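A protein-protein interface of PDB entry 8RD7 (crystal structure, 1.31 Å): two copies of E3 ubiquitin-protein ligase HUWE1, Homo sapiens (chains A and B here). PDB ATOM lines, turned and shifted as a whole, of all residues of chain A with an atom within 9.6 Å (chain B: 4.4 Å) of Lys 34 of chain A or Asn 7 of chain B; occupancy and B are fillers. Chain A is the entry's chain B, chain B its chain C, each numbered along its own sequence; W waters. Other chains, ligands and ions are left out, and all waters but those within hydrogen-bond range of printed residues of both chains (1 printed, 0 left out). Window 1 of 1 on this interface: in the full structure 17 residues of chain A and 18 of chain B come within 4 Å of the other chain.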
ATOM      1  N   ASN A   7      13.721 -20.921 -10.096  1.00  0.00           N
ATOM      2  CA  ASN A   7      14.664 -21.260  -9.047  1.00  0.00           C
ATOM      3  C   ASN A   7      15.822 -22.153  -9.475  1.00  0.00           C
ATOM      4  O   ASN A   7      16.844 -22.172  -8.778  1.00  0.00           O
ATOM      5  CB  ASN A   7      13.930 -21.893  -7.863  1.00  0.00           C
ATOM      6  CG  ASN A   7      13.176 -23.167  -8.234  1.00  0.00           C
ATOM      7  OD1 ASN A   7      12.527 -23.256  -9.293  1.00  0.00           O
ATOM      8  ND2 ASN A   7      13.221 -24.160  -7.321  1.00  0.00           N
ATOM      9  N   TRP A   8      15.749 -22.829 -10.629  1.00  0.00           N
ATOM     10  CA  TRP A   8      16.877 -23.619 -11.129  1.00  0.00           C
ATOM     11  C   TRP A   8      17.704 -22.791 -12.088  1.00  0.00           C
ATOM     12  O   TRP A   8      17.199 -21.853 -12.736  1.00  0.00           O
ATOM     13  CB  TRP A   8      16.371 -24.865 -11.866  1.00  0.00           C
ATOM     14  CG  TRP A   8      15.904 -25.887 -10.885  1.00  0.00           C
ATOM     15  CD1 TRP A   8      14.655 -25.962 -10.283  1.00  0.00           C
ATOM     16  CD2 TRP A   8      16.680 -26.953 -10.327  1.00  0.00           C
ATOM     17  NE1 TRP A   8      14.616 -27.030  -9.401  1.00  0.00           N
ATOM     18  CE2 TRP A   8      15.841 -27.655  -9.420  1.00  0.00           C
ATOM     19  CE3 TRP A   8      18.010 -27.376 -10.491  1.00  0.00           C
ATOM     20  CZ2 TRP A   8      16.290 -28.762  -8.695  1.00  0.00           C
ATOM     21  CZ3 TRP A   8      18.447 -28.479  -9.783  1.00  0.00           C
ATOM     22  CH2 TRP A   8      17.591 -29.156  -8.884  1.00  0.00           C
ATOM     23  N   ASN A  26      11.763 -24.878 -16.127  1.00  0.00           N
ATOM     24  CA  ASN A  26      11.965 -24.808 -14.687  1.00  0.00           C
ATOM     25  C   ASN A  26      10.925 -25.644 -13.951  1.00  0.00           C
ATOM     26  O   ASN A  26      11.261 -26.396 -13.024  1.00  0.00           O
ATOM     27  CB  ASN A  26      11.927 -23.357 -14.220  1.00  0.00           C
ATOM     28  CG  ASN A  26      12.378 -23.209 -12.790  1.00  0.00           C
ATOM     29  OD1 ASN A  26      13.569 -23.125 -12.547  1.00  0.00           O
ATOM     30  ND2 ASN A  26      11.442 -23.231 -11.840  1.00  0.00           N
ATOM     31  N   SER A  27       9.658 -25.571 -14.386  1.00  0.00           N
ATOM     32  CA  SER A  27       8.613 -26.334 -13.722  1.00  0.00           C
ATOM     33  C   SER A  27       8.808 -27.839 -13.926  1.00  0.00           C
ATOM     34  O   SER A  27       8.624 -28.624 -12.991  1.00  0.00           O
ATOM     35  CB  SER A  27       7.241 -25.841 -14.186  1.00  0.00           C
ATOM     36  OG  SER A  27       6.200 -26.646 -13.664  1.00  0.00           O
ATOM     37  N   THR A  28       9.216 -28.255 -15.135  1.00  0.00           N
ATOM     38  CA  THR A  28       9.484 -29.666 -15.389  1.00  0.00           C
ATOM     39  C   THR A  28      10.610 -30.169 -14.489  1.00  0.00           C
ATOM     40  O   THR A  28      10.493 -31.230 -13.859  1.00  0.00           O
ATOM     41  CB  THR A  28       9.858 -29.852 -16.864  1.00  0.00           C
ATOM     42  OG1 THR A  28       8.739 -29.524 -17.698  1.00  0.00           O
ATOM     43  CG2 THR A  28      10.273 -31.322 -17.164  1.00  0.00           C
ATOM     44  N   ILE A  29      11.699 -29.404 -14.402  1.00  0.00           N
ATOM     45  CA  ILE A  29      12.824 -29.792 -13.553  1.00  0.00           C
ATOM     46  C   ILE A  29      12.404 -29.810 -12.089  1.00  0.00           C
ATOM     47  O   ILE A  29      12.669 -30.776 -11.360  1.00  0.00           O
ATOM     48  CB  ILE A  29      14.024 -28.854 -13.794  1.00  0.00           C
ATOM     49  CG1 ILE A  29      14.568 -29.037 -15.214  1.00  0.00           C
ATOM     50  CG2 ILE A  29      15.138 -29.092 -12.772  1.00  0.00           C
ATOM     51  CD1 ILE A  29      15.482 -27.901 -15.602  1.00  0.00           C
ATOM     52  N   ASP A  30      11.740 -28.738 -11.631  1.00  0.00           N
ATOM     53  CA  ASP A  30      11.427 -28.636 -10.209  1.00  0.00           C
ATOM     54  C   ASP A  30      10.403 -29.679  -9.791  1.00  0.00           C
ATOM     55  O   ASP A  30      10.451 -30.172  -8.655  1.00  0.00           O
ATOM     56  CB  ASP A  30      10.911 -27.245  -9.867  1.00  0.00           C
ATOM     57  CG  ASP A  30      11.022 -26.942  -8.399  1.00  0.00           C
ATOM     58  OD1 ASP A  30      12.148 -27.105  -7.864  1.00  0.00           O
ATOM     59  OD2 ASP A  30       9.997 -26.543  -7.801  1.00  0.00           O
ATOM     60  N   SER A  31       9.488 -30.051 -10.692  1.00  0.00           N
ATOM     61  CA  SER A  31       8.527 -31.093 -10.347  1.00  0.00           C
ATOM     62  C   SER A  31       9.219 -32.433 -10.158  1.00  0.00           C
ATOM     63  O   SER A  31       8.873 -33.194  -9.241  1.00  0.00           O
ATOM     64  CB  SER A  31       7.478 -31.209 -11.440  1.00  0.00           C
ATOM     65  OG  SER A  31       6.643 -30.063 -11.444  1.00  0.00           O
ATOM     66  N   ALA A  32      10.200 -32.742 -11.025  1.00  0.00           N
ATOM     67  CA  ALA A  32      10.945 -33.984 -10.869  1.00  0.00           C
ATOM     68  C   ALA A  32      11.798 -33.940  -9.607  1.00  0.00           C
ATOM     69  O   ALA A  32      11.928 -34.948  -8.891  1.00  0.00           O
ATOM     70  CB  ALA A  32      11.813 -34.230 -12.106  1.00  0.00           C
ATOM     71  N   TRP A  33      12.363 -32.771  -9.307  1.00  0.00           N
ATOM     72  CA  TRP A  33      13.121 -32.633  -8.065  1.00  0.00           C
ATOM     73  C   TRP A  33      12.241 -32.961  -6.866  1.00  0.00           C
ATOM     74  O   TRP A  33      12.607 -33.775  -6.013  1.00  0.00           O
ATOM     75  CB  TRP A  33      13.677 -31.204  -7.951  1.00  0.00           C
ATOM     76  CG  TRP A  33      14.401 -30.956  -6.634  1.00  0.00           C
ATOM     77  CD1 TRP A  33      13.959 -30.232  -5.559  1.00  0.00           C
ATOM     78  CD2 TRP A  33      15.681 -31.460  -6.283  1.00  0.00           C
ATOM     79  NE1 TRP A  33      14.918 -30.235  -4.572  1.00  0.00           N
ATOM     80  CE2 TRP A  33      15.970 -31.010  -4.983  1.00  0.00           C
ATOM     81  CE3 TRP A  33      16.628 -32.245  -6.960  1.00  0.00           C
ATOM     82  CZ2 TRP A  33      17.174 -31.298  -4.351  1.00  0.00           C
ATOM     83  CZ3 TRP A  33      17.813 -32.543  -6.336  1.00  0.00           C
ATOM     84  CH2 TRP A  33      18.078 -32.070  -5.032  1.00  0.00           C
ATOM     85  N   LYS A  34      11.052 -32.362  -6.808  1.00  0.00           N
ATOM     86  CA  LYS A  34      10.179 -32.555  -5.653  1.00  0.00           C
ATOM     87  C   LYS A  34       9.644 -33.979  -5.545  1.00  0.00           C
ATOM     88  O   LYS A  34       9.316 -34.423  -4.442  1.00  0.00           O
ATOM     89  CB  LYS A  34       9.097 -31.473  -5.626  1.00  0.00           C
ATOM     90  CG  LYS A  34       9.688 -30.096  -5.289  1.00  0.00           C
ATOM     91  CD  LYS A  34       8.709 -28.905  -5.362  1.00  0.00           C
ATOM     92  CE  LYS A  34       8.662 -28.133  -4.005  1.00  0.00           C
ATOM     93  NZ  LYS A  34       9.952 -27.525  -3.478  1.00  0.00           N
ATOM     94  N   SER A  35       9.592 -34.718  -6.651  1.00  0.00           N
ATOM     95  CA  SER A  35       9.080 -36.079  -6.667  1.00  0.00           C
ATOM     96  C   SER A  35      10.130 -37.122  -6.318  1.00  0.00           C
ATOM     97  O   SER A  35       9.818 -38.313  -6.323  1.00  0.00           O
ATOM     98  CB  SER A  35       8.574 -36.396  -8.067  1.00  0.00           C
ATOM     99  OG  SER A  35       7.527 -35.504  -8.412  1.00  0.00           O
ATOM    100  N   GLY A  36      11.358 -36.723  -6.028  1.00  0.00           N
ATOM    101  CA  GLY A  36      12.390 -37.671  -5.657  1.00  0.00           C
ATOM    102  C   GLY A  36      13.096 -38.360  -6.803  1.00  0.00           C
ATOM    103  O   GLY A  36      13.938 -39.234  -6.542  1.00  0.00           O
ATOM    104  N   GLU A  37      12.793 -37.999  -8.051  1.00  0.00           N
ATOM    105  CA  GLU A  37      13.433 -38.626  -9.201  1.00  0.00           C
ATOM    106  C   GLU A  37      14.932 -38.332  -9.186  1.00  0.00           C
ATOM    107  O   GLU A  37      15.377 -37.276  -8.721  1.00  0.00           O
ATOM    108  CB  GLU A  37      12.874 -38.006 -10.490  1.00  0.00           C
ATOM    109  CG  GLU A  37      11.365 -38.046 -10.599  1.00  0.00           C
ATOM    110  CD  GLU A  37      10.905 -39.128 -11.509  1.00  0.00           C
ATOM    111  OE1 GLU A  37      11.788 -39.787 -12.121  1.00  0.00           O
ATOM    112  OE2 GLU A  37       9.667 -39.322 -11.613  1.00  0.00           O
ATOM    113  N   THR A  38      15.731 -39.252  -9.734  1.00  0.00           N
ATOM    114  CA  THR A  38      17.172 -39.004  -9.796  1.00  0.00           C
ATOM    115  C   THR A  38      17.597 -38.205 -11.027  1.00  0.00           C
ATOM    116  O   THR A  38      18.716 -37.670 -11.058  1.00  0.00           O
ATOM    117  CB  THR A  38      17.974 -40.305  -9.750  1.00  0.00           C
ATOM    118  OG1 THR A  38      17.491 -41.193 -10.764  1.00  0.00           O
ATOM    119  CG2 THR A  38      17.796 -40.990  -8.411  1.00  0.00           C
ATOM    120  N   SER A  39      16.744 -38.102 -12.042  1.00  0.00           N
ATOM    121  CA  SER A  39      17.070 -37.326 -13.239  1.00  0.00           C
ATOM    122  C   SER A  39      15.756 -36.906 -13.879  1.00  0.00           C
ATOM    123  O   SER A  39      14.676 -37.411 -13.529  1.00  0.00           O
ATOM    124  CB  SER A  39      17.926 -38.134 -14.232  1.00  0.00           C
ATOM    125  OG  SER A  39      17.225 -39.265 -14.751  1.00  0.00           O
ATOM    126  N   VAL A  40      15.861 -36.002 -14.853  1.00  0.00           N
ATOM    127  CA  VAL A  40      14.685 -35.539 -15.574  1.00  0.00           C
ATOM    128  C   VAL A  40      15.101 -35.129 -16.982  1.00  0.00           C
ATOM    129  O   VAL A  40      16.153 -34.514 -17.183  1.00  0.00           O
ATOM    130  CB  VAL A  40      13.992 -34.382 -14.827  1.00  0.00           C
ATOM    131  CG1 VAL A  40      14.959 -33.206 -14.634  1.00  0.00           C
ATOM    132  CG2 VAL A  40      12.698 -33.949 -15.566  1.00  0.00           C
ATOM    133  N   PHE A  53      20.306 -35.224 -11.210  1.00  0.00           N
ATOM    134  CA  PHE A  53      20.284 -34.663  -9.869  1.00  0.00           C
ATOM    135  C   PHE A  53      21.335 -35.272  -8.957  1.00  0.00           C
ATOM    136  O   PHE A  53      21.650 -34.668  -7.922  1.00  0.00           O
ATOM    137  CB  PHE A  53      18.913 -34.890  -9.269  1.00  0.00           C
ATOM    138  CG  PHE A  53      17.808 -34.095  -9.931  1.00  0.00           C
ATOM    139  CD1 PHE A  53      17.955 -32.741 -10.206  1.00  0.00           C
ATOM    140  CD2 PHE A  53      16.589 -34.713 -10.213  1.00  0.00           C
ATOM    141  CE1 PHE A  53      16.937 -32.029 -10.774  1.00  0.00           C
ATOM    142  CE2 PHE A  53      15.518 -33.991 -10.742  1.00  0.00           C
ATOM    143  CZ  PHE A  53      15.693 -32.650 -11.041  1.00  0.00           C
ATOM    144  N   LEU A  71      20.383 -25.153  -7.581  1.00  0.00           N
ATOM    145  CA  LEU A  71      19.061 -24.877  -7.054  1.00  0.00           C
ATOM    146  C   LEU A  71      19.242 -23.678  -6.141  1.00  0.00           C
ATOM    147  O   LEU A  71      19.998 -23.741  -5.160  1.00  0.00           O
ATOM    148  CB  LEU A  71      18.570 -26.113  -6.301  1.00  0.00           C
ATOM    149  CG  LEU A  71      17.299 -25.955  -5.487  1.00  0.00           C
ATOM    150  CD1 LEU A  71      16.166 -25.444  -6.388  1.00  0.00           C
ATOM    151  CD2 LEU A  71      16.897 -27.335  -4.952  1.00  0.00           C
ATOM    152  N   THR A  72      18.602 -22.569  -6.487  1.00  0.00           N
ATOM    153  CA  THR A  72      18.677 -21.416  -5.620  1.00  0.00           C
ATOM    154  C   THR A  72      17.874 -21.679  -4.336  1.00  0.00           C
ATOM    155  O   THR A  72      16.891 -22.445  -4.317  1.00  0.00           O
ATOM    156  CB  THR A  72      18.233 -20.148  -6.361  1.00  0.00           C
ATOM    157  OG1 THR A  72      16.866 -20.264  -6.723  1.00  0.00           O
ATOM    158  CG2 THR A  72      19.033 -19.960  -7.630  1.00  0.00           C
ATOM    159  N   LEU A  73      18.334 -21.106  -3.241  1.00  0.00           N
ATOM    160  CA  LEU A  73      17.672 -21.308  -1.964  1.00  0.00           C
ATOM    161  C   LEU A  73      17.332 -19.973  -1.353  1.00  0.00           C
ATOM    162  O   LEU A  73      18.213 -19.096  -1.259  1.00  0.00           O
ATOM    163  CB  LEU A  73      18.624 -21.957  -1.027  1.00  0.00           C
ATOM    164  CG  LEU A  73      18.980 -23.340  -1.463  1.00  0.00           C
ATOM    165  CD1 LEU A  73      20.062 -23.808  -0.531  1.00  0.00           C
ATOM    166  CD2 LEU A  73      17.739 -24.265  -1.510  1.00  0.00           C
ATOM    167  N   ASN B   6       4.535 -32.391  -0.903  1.00  0.00           N
ATOM    168  CA  ASN B   6       4.197 -31.835   0.403  1.00  0.00           C
ATOM    169  C   ASN B   6       5.404 -31.603   1.303  1.00  0.00           C
ATOM    170  O   ASN B   6       5.802 -32.450   2.110  1.00  0.00           O
ATOM    171  CB  ASN B   6       3.132 -32.661   1.111  1.00  0.00           C
ATOM    172  CG  ASN B   6       1.738 -32.286   0.666  1.00  0.00           C
ATOM    173  OD1 ASN B   6       1.553 -31.755  -0.451  1.00  0.00           O
ATOM    174  ND2 ASN B   6       0.741 -32.548   1.528  1.00  0.00           N
ATOM    175  N   ASN B   7       5.939 -30.393   1.193  1.00  0.00           N
ATOM    176  CA  ASN B   7       7.204 -30.039   1.802  1.00  0.00           C
ATOM    177  C   ASN B   7       7.078 -29.123   3.022  1.00  0.00           C
ATOM    178  O   ASN B   7       8.054 -29.010   3.768  1.00  0.00           O
ATOM    179  CB  ASN B   7       8.105 -29.406   0.736  1.00  0.00           C
ATOM    180  CG  ASN B   7       7.479 -28.179   0.113  1.00  0.00           C
ATOM    181  OD1 ASN B   7       6.269 -28.137  -0.163  1.00  0.00           O
ATOM    182  ND2 ASN B   7       8.312 -27.168  -0.148  1.00  0.00           N
ATOM    183  N   TRP B   8       5.924 -28.499   3.274  1.00  0.00           N
ATOM    184  CA  TRP B   8       5.748 -27.684   4.475  1.00  0.00           C
ATOM    185  C   TRP B   8       5.191 -28.532   5.595  1.00  0.00           C
ATOM    186  O   TRP B   8       4.474 -29.520   5.351  1.00  0.00           O
ATOM    187  CB  TRP B   8       4.814 -26.484   4.216  1.00  0.00           C
ATOM    188  CG  TRP B   8       5.528 -25.428   3.431  1.00  0.00           C
ATOM    189  CD1 TRP B   8       5.668 -25.369   2.070  1.00  0.00           C
ATOM    190  CD2 TRP B   8       6.234 -24.299   3.960  1.00  0.00           C
ATOM    191  NE1 TRP B   8       6.424 -24.264   1.719  1.00  0.00           N
ATOM    192  CE2 TRP B   8       6.791 -23.599   2.865  1.00  0.00           C
ATOM    193  CE3 TRP B   8       6.434 -23.799   5.260  1.00  0.00           C
ATOM    194  CZ2 TRP B   8       7.544 -22.433   3.033  1.00  0.00           C
ATOM    195  CZ3 TRP B   8       7.196 -22.638   5.427  1.00  0.00           C
ATOM    196  CH2 TRP B   8       7.744 -21.971   4.315  1.00  0.00           C
ATOM    197  N   ARG B   9       5.555 -28.184   6.843  1.00  0.00           N
ATOM    198  CA  ARG B   9       5.006 -28.897   7.994  1.00  0.00           C
ATOM    199  C   ARG B   9       4.675 -27.934   9.125  1.00  0.00           C
ATOM    200  O   ARG B   9       5.298 -26.873   9.250  1.00  0.00           O
ATOM    201  CB  ARG B   9       6.032 -29.874   8.590  1.00  0.00           C
ATOM    202  CG  ARG B   9       6.620 -30.870   7.577  1.00  0.00           C
ATOM    203  CD  ARG B   9       5.808 -32.164   7.529  1.00  0.00           C
ATOM    204  NE  ARG B   9       6.502 -33.187   6.749  1.00  0.00           N
ATOM    205  CZ  ARG B   9       6.490 -33.267   5.419  1.00  0.00           C
ATOM    206  NH1 ARG B   9       5.805 -32.403   4.674  1.00  0.00           N
ATOM    207  NH2 ARG B   9       7.194 -34.230   4.815  1.00  0.00           N
ATOM    208  N   ASN B  26      -0.734 -26.972   1.075  1.00  0.00           N
ATOM    209  CA  ASN B  26       0.705 -26.930   0.867  1.00  0.00           C
ATOM    210  C   ASN B  26       1.036 -26.124  -0.384  1.00  0.00           C
ATOM    211  O   ASN B  26       1.977 -25.324  -0.387  1.00  0.00           O
ATOM    212  CB  ASN B  26       1.243 -28.348   0.724  1.00  0.00           C
ATOM    213  CG  ASN B  26       2.745 -28.396   0.767  1.00  0.00           C
ATOM    214  OD1 ASN B  26       3.323 -28.440   1.850  1.00  0.00           O
ATOM    215  ND2 ASN B  26       3.391 -28.307  -0.400  1.00  0.00           N
ATOM    216  N   ASP B  30       3.302 -22.920  -0.466  1.00  0.00           N
ATOM    217  CA  ASP B  30       4.562 -22.995  -1.197  1.00  0.00           C
ATOM    218  C   ASP B  30       4.596 -21.973  -2.329  1.00  0.00           C
ATOM    219  O   ASP B  30       5.662 -21.434  -2.641  1.00  0.00           O
ATOM    220  CB  ASP B  30       4.795 -24.417  -1.703  1.00  0.00           C
ATOM    221  CG  ASP B  30       6.241 -24.692  -2.015  1.00  0.00           C
ATOM    222  OD1 ASP B  30       7.098 -24.413  -1.139  1.00  0.00           O
ATOM    223  OD2 ASP B  30       6.515 -25.221  -3.108  1.00  0.00           O
ATOM    224  N   LYS B  34       7.524 -19.129  -2.721  1.00  0.00           N
ATOM    225  CA  LYS B  34       8.373 -18.968  -3.900  1.00  0.00           C
ATOM    226  C   LYS B  34       8.225 -17.563  -4.497  1.00  0.00           C
ATOM    227  O   LYS B  34       9.137 -17.068  -5.171  1.00  0.00           O
ATOM    228  CB  LYS B  34       7.953 -20.003  -4.942  1.00  0.00           C
ATOM    229  CG  LYS B  34       8.136 -21.512  -4.615  1.00  0.00           C
ATOM    230  CD  LYS B  34       7.366 -22.363  -5.708  1.00  0.00           C
ATOM    231  CE  LYS B  34       7.572 -23.900  -5.643  1.00  0.00           C
ATOM    232  NZ  LYS B  34       8.993 -24.322  -5.708  1.00  0.00           N
ATOM    233  N   MET B  70       7.769 -25.478   9.512  1.00  0.00           N
ATOM    234  CA  MET B  70       9.071 -25.692   8.919  1.00  0.00           C
ATOM    235  C   MET B  70       8.933 -26.038   7.436  1.00  0.00           C
ATOM    236  O   MET B  70       7.896 -26.533   6.980  1.00  0.00           O
ATOM    237  CB  MET B  70       9.865 -26.759   9.639  1.00  0.00           C
ATOM    238  CG  MET B  70       9.318 -28.119   9.475  1.00  0.00           C
ATOM    239  SD  MET B  70      10.476 -29.416  10.020  1.00  0.00           S
ATOM    240  CE  MET B  70      11.637 -29.478   8.718  1.00  0.00           C
ATOM    241  N   LEU B  71      10.002 -25.788   6.700  1.00  0.00           N
ATOM    242  CA  LEU B  71      10.116 -26.124   5.293  1.00  0.00           C
ATOM    243  C   LEU B  71      11.125 -27.253   5.207  1.00  0.00           C
ATOM    244  O   LEU B  71      12.271 -27.100   5.628  1.00  0.00           O
ATOM    245  CB  LEU B  71      10.635 -24.900   4.548  1.00  0.00           C
ATOM    246  CG  LEU B  71      11.027 -25.065   3.097  1.00  0.00           C
ATOM    247  CD1 LEU B  71       9.799 -25.576   2.317  1.00  0.00           C
ATOM    248  CD2 LEU B  71      11.493 -23.719   2.549  1.00  0.00           C
ATOM    249  N   THR B  72      10.689 -28.412   4.746  1.00  0.00           N
ATOM    250  CA  THR B  72      11.628 -29.500   4.589  1.00  0.00           C
ATOM    251  C   THR B  72      12.562 -29.192   3.417  1.00  0.00           C
ATOM    252  O   THR B  72      12.213 -28.465   2.475  1.00  0.00           O
ATOM    253  CB  THR B  72      10.886 -30.820   4.415  1.00  0.00           C
ATOM    254  OG1 THR B  72      10.152 -30.779   3.208  1.00  0.00           O
ATOM    255  CG2 THR B  72       9.871 -31.025   5.534  1.00  0.00           C
HETATM  256  O   HOH W   1       9.624 -24.897  -2.005  1.00  0.00           O
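Water W1 lies within hydrogen-bond range of the side-chain carboxylate (OD1) of Asp 30 of chain B, the side-chain amino group (NZ) of Lys 34 of chain A and the side-chain amide nitrogen (ND2) of Asn 7 of chain B.
Printed residues of chain B within 4 Å of Asp 30 of chain A: Lys 34.
Trp 33 of chain A touches none of the printed residues of chain B.
Printed residues of chain B within 4 Å of Lys 34 of chain A: Asn 7 (3.7 Å) and Asp 30 (3.7 Å).
Leu 71 of chain A touches none of the printed residues of chain B.
Printed residues of chain A within 4 Å of Asp 30 of chain B: Lys 34.
Of the printed residues of chain A, Lys 34 of chain B touches Asp 30.
No residue of chain A comes within 4 Å of Thr 72 of chain B.
The nearest residue of chain A that does not touch Asn 7 of chain B is Asp 30 of chain A (7.9 Å).
The nearest printed residue of chain A that does not touch Asp 30 of chain B is Asp 30 of chain A (6.0 Å).
Asn 7 of chain B touches Lys 34 of chain A (ND2 to NZ, 3.7 Å).
CE of Lys 34 of chain A touches OD2 of Asp 30 of chain B, at 3.7 Å.
Asp 30 of chain A touches Lys 34 of chain B, and with the chains exchanged Lys 34 of chain A touches Asp 30 of chain B.
Lys 34 of chain A touches Asn 7 of chain B, but with the chains exchanged Asn 7 of chain A does not touch Lys 34 of chain B (4.5 Å).
Of the 3 pairs that touch across the chains among the printed residues, 2 have their exchanged pair printed and touching as well.
Of the 10 printed residues of chain B, 3 touch a printed residue of chain A.
Of the 21 printed residues of chain A, 2 touch a printed residue of chain B.
Among the printed residues, 3 pairs touch across the chains.
Among the printed residues, Asp or Glu carboxylates within 4 Å of a Lys or Arg side-chain nitrogen of the other chain: Asp 30 of chain A with Lys 34 of chain B.
NZ of Lys 34 of chain B lies within salt-bridge range of OD2 of Asp 30 of chain A.
OD1 of Asp 30 of chain A lies within hydrogen-bond range of ND2 of Asn 7 of chain A, at 3.2 Å.
ND2 of Asn 26 of chain B sits at hydrogen-bond distance from OD1 of Asn 7 of chain B, 2.9 Å away.
The side-chain amide nitrogen (ND2) of Asn 7 of chain B is in hydrogen-bond range of the side-chain carboxylate (OD1) of Asp 30 of chain B (3.2 Å).
O of Asn 7 of chain B sits at hydrogen-bond distance from OG1 of Thr 72 of chain B.
The indole nitrogen (NE1) of Trp 8 of chain B lies within hydrogen-bond range of the side-chain carboxylate (OD1) of Asp 30 of chain B, at 2.9 Å.
OD2 of Asp 30 of chain B lies within salt-bridge range of NZ of Lys 34 of chain B (3.7 Å).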
